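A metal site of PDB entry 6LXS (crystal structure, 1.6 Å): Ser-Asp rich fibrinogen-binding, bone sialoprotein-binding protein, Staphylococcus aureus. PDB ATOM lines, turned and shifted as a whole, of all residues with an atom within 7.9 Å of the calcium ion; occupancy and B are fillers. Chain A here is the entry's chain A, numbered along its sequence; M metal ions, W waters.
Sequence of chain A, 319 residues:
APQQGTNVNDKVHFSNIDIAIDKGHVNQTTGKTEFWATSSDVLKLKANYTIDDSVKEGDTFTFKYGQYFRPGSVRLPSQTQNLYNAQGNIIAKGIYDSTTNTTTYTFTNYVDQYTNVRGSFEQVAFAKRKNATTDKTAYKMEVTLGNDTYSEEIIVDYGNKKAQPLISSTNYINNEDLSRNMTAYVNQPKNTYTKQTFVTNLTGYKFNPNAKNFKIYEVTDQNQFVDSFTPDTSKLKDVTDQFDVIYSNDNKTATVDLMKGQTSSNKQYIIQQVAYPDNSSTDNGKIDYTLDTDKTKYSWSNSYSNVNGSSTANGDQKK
Of the 11 residues printed, 3 come within 4 Å of the calcium ion.
The calcium ion is bound by O of Ile 19 (2.3 Å), water W1 (2.4 Å), OD1 of Asp 18 (2.4 Å), OE2 of Glu 152 (2.5 Å) and OE1 of Glu 152 (2.5 Å).
The calcium ion has five donor atoms within binding distance.
OD1 of Asp 18 sits close to OH of Tyr 150 (3.5 Å).
The side-chain carboxylate (OE1) of Glu 152 lies close to the side-chain hydroxyl (OH) of Tyr 150 (2.5 Å).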
ATOM      1  N   ILE A  17     -28.159  11.613  10.415  1.00  0.00           N
ATOM      2  CA  ILE A  17     -26.751  11.845   9.990  1.00  0.00           C
ATOM      3  C   ILE A  17     -26.071  12.730  11.031  1.00  0.00           C
ATOM      4  O   ILE A  17     -26.619  13.725  11.492  1.00  0.00           O
ATOM      5  CB  ILE A  17     -26.644  12.444   8.604  1.00  0.00           C
ATOM      6  CG1 ILE A  17     -27.424  11.603   7.606  1.00  0.00           C
ATOM      7  CG2 ILE A  17     -25.167  12.478   8.193  1.00  0.00           C
ATOM      8  CD1 ILE A  17     -27.585  12.321   6.277  1.00  0.00           C
ATOM      9  N   ASP A  18     -24.854  12.363  11.452  1.00  0.00           N
ATOM     10  CA  ASP A  18     -24.105  13.224  12.410  1.00  0.00           C
ATOM     11  C   ASP A  18     -22.597  13.051  12.077  1.00  0.00           C
ATOM     12  O   ASP A  18     -22.189  11.979  11.584  1.00  0.00           O
ATOM     13  CB  ASP A  18     -24.305  12.761  13.839  1.00  0.00           C
ATOM     14  CG  ASP A  18     -23.960  13.852  14.892  1.00  0.00           C
ATOM     15  OD1 ASP A  18     -23.472  14.938  14.575  1.00  0.00           O
ATOM     16  OD2 ASP A  18     -24.293  13.601  16.095  1.00  0.00           O
ATOM     17  N   ILE A  19     -21.851  14.084  12.402  1.00  0.00           N
ATOM     18  CA  ILE A  19     -20.368  14.072  12.393  1.00  0.00           C
ATOM     19  C   ILE A  19     -19.951  14.322  13.856  1.00  0.00           C
ATOM     20  O   ILE A  19     -20.298  15.317  14.458  1.00  0.00           O
ATOM     21  CB  ILE A  19     -19.775  15.108  11.456  1.00  0.00           C
ATOM     22  CG1 ILE A  19     -20.208  14.813  10.020  1.00  0.00           C
ATOM     23  CG2 ILE A  19     -18.261  15.146  11.630  1.00  0.00           C
ATOM     24  CD1 ILE A  19     -19.827  15.863   8.986  1.00  0.00           C
ATOM     25  N   ALA A  20     -19.241  13.305  14.358  1.00  0.00           N
ATOM     26  CA  ALA A  20     -18.734  13.386  15.696  1.00  0.00           C
ATOM     27  C   ALA A  20     -17.255  13.704  15.692  1.00  0.00           C
ATOM     28  O   ALA A  20     -16.575  13.422  14.711  1.00  0.00           O
ATOM     29  CB  ALA A  20     -18.945  12.111  16.456  1.00  0.00           C
ATOM     30  N   ILE A  21     -16.827  14.321  16.793  1.00  0.00           N
ATOM     31  CA  ILE A  21     -15.375  14.520  17.060  1.00  0.00           C
ATOM     32  C   ILE A  21     -15.034  13.509  18.149  1.00  0.00           C
ATOM     33  O   ILE A  21     -15.626  13.559  19.170  1.00  0.00           O
ATOM     34  CB  ILE A  21     -15.008  15.936  17.513  1.00  0.00           C
ATOM     35  CG1 ILE A  21     -15.690  17.004  16.658  1.00  0.00           C
ATOM     36  CG2 ILE A  21     -13.498  16.084  17.487  1.00  0.00           C
ATOM     37  CD1 ILE A  21     -15.476  18.397  17.147  1.00  0.00           C
ATOM     38  N   LYS A  44     -15.934  11.217  13.095  1.00  0.00           N
ATOM     39  CA  LYS A  44     -16.697  10.054  12.755  1.00  0.00           C
ATOM     40  C   LYS A  44     -17.988  10.460  12.040  1.00  0.00           C
ATOM     41  O   LYS A  44     -18.751  11.269  12.566  1.00  0.00           O
ATOM     42  CB  LYS A  44     -17.097   9.346  14.035  1.00  0.00           C
ATOM     43  CG  LYS A  44     -15.930   8.744  14.800  1.00  0.00           C
ATOM     44  CD  LYS A  44     -15.454   7.407  14.303  1.00  0.00           C
ATOM     45  CE  LYS A  44     -14.552   6.748  15.367  1.00  0.00           C
ATOM     46  NZ  LYS A  44     -15.404   5.983  16.332  1.00  0.00           N
ATOM     47  N   TYR A 150     -25.804  16.594   4.510  1.00  0.00           N
ATOM     48  CA  TYR A 150     -25.635  16.982   5.916  1.00  0.00           C
ATOM     49  C   TYR A 150     -24.356  17.795   6.042  1.00  0.00           C
ATOM     50  O   TYR A 150     -23.364  17.551   5.354  1.00  0.00           O
ATOM     51  CB  TYR A 150     -25.482  15.726   6.811  1.00  0.00           C
ATOM     52  CG  TYR A 150     -25.264  16.071   8.248  1.00  0.00           C
ATOM     53  CD1 TYR A 150     -26.259  16.439   9.064  1.00  0.00           C
ATOM     54  CD2 TYR A 150     -23.968  16.067   8.761  1.00  0.00           C
ATOM     55  CE1 TYR A 150     -26.037  16.861  10.335  1.00  0.00           C
ATOM     56  CE2 TYR A 150     -23.723  16.450  10.078  1.00  0.00           C
ATOM     57  CZ  TYR A 150     -24.763  16.815  10.889  1.00  0.00           C
ATOM     58  OH  TYR A 150     -24.576  17.194  12.186  1.00  0.00           O
ATOM     59  N   SER A 151     -24.399  18.745   6.948  1.00  0.00           N
ATOM     60  CA  SER A 151     -23.154  19.468   7.288  1.00  0.00           C
ATOM     61  C   SER A 151     -23.225  20.024   8.704  1.00  0.00           C
ATOM     62  O   SER A 151     -24.276  20.165   9.233  1.00  0.00           O
ATOM     63  CB  SER A 151     -22.854  20.534   6.309  1.00  0.00           C
ATOM     64  OG  SER A 151     -23.704  21.603   6.525  1.00  0.00           O
ATOM     65  N   GLU A 152     -22.056  20.166   9.308  1.00  0.00           N
ATOM     66  CA  GLU A 152     -21.933  20.900  10.540  1.00  0.00           C
ATOM     67  C   GLU A 152     -20.549  21.574  10.553  1.00  0.00           C
ATOM     68  O   GLU A 152     -19.612  21.107   9.870  1.00  0.00           O
ATOM     69  CB  GLU A 152     -22.197  20.085  11.806  1.00  0.00           C
ATOM     70  CG  GLU A 152     -21.100  19.226  12.210  1.00  0.00           C
ATOM     71  CD  GLU A 152     -21.452  18.319  13.373  1.00  0.00           C
ATOM     72  OE1 GLU A 152     -22.248  17.332  13.202  1.00  0.00           O
ATOM     73  OE2 GLU A 152     -20.842  18.534  14.496  1.00  0.00           O
ATOM     74  N   GLU A 153     -20.471  22.670  11.304  1.00  0.00           N
ATOM     75  CA  GLU A 153     -19.221  23.418  11.455  1.00  0.00           C
ATOM     76  C   GLU A 153     -18.348  22.756  12.479  1.00  0.00           C
ATOM     77  O   GLU A 153     -18.817  22.534  13.640  1.00  0.00           O
ATOM     78  CB  GLU A 153     -19.540  24.879  11.920  1.00  0.00           C
ATOM     79  CG  GLU A 153     -20.386  25.591  10.911  1.00  0.00           C
ATOM     80  CD  GLU A 153     -19.579  26.525  10.112  1.00  0.00           C
ATOM     81  OE1 GLU A 153     -19.554  26.384   8.871  1.00  0.00           O
ATOM     82  OE2 GLU A 153     -19.017  27.447  10.757  1.00  0.00           O
ATOM     83  N   ILE A 154     -17.067  22.509  12.126  1.00  0.00           N
ATOM     84  CA  ILE A 154     -16.096  21.882  13.054  1.00  0.00           C
ATOM     85  C   ILE A 154     -14.922  22.850  13.085  1.00  0.00           C
ATOM     86  O   ILE A 154     -14.335  23.131  12.069  1.00  0.00           O
ATOM     87  CB  ILE A 154     -15.628  20.517  12.552  1.00  0.00           C
ATOM     88  CG1 ILE A 154     -16.803  19.520  12.464  1.00  0.00           C
ATOM     89  CG2 ILE A 154     -14.449  20.006  13.425  1.00  0.00           C
ATOM     90  CD1 ILE A 154     -17.454  19.161  13.712  1.00  0.00           C
HETATM   91 CA    CA M   1     -21.909  16.528  15.561  1.00  0.00          CA
HETATM   92  O   HOH W   1     -22.388  14.982  17.321  1.00  0.00           O
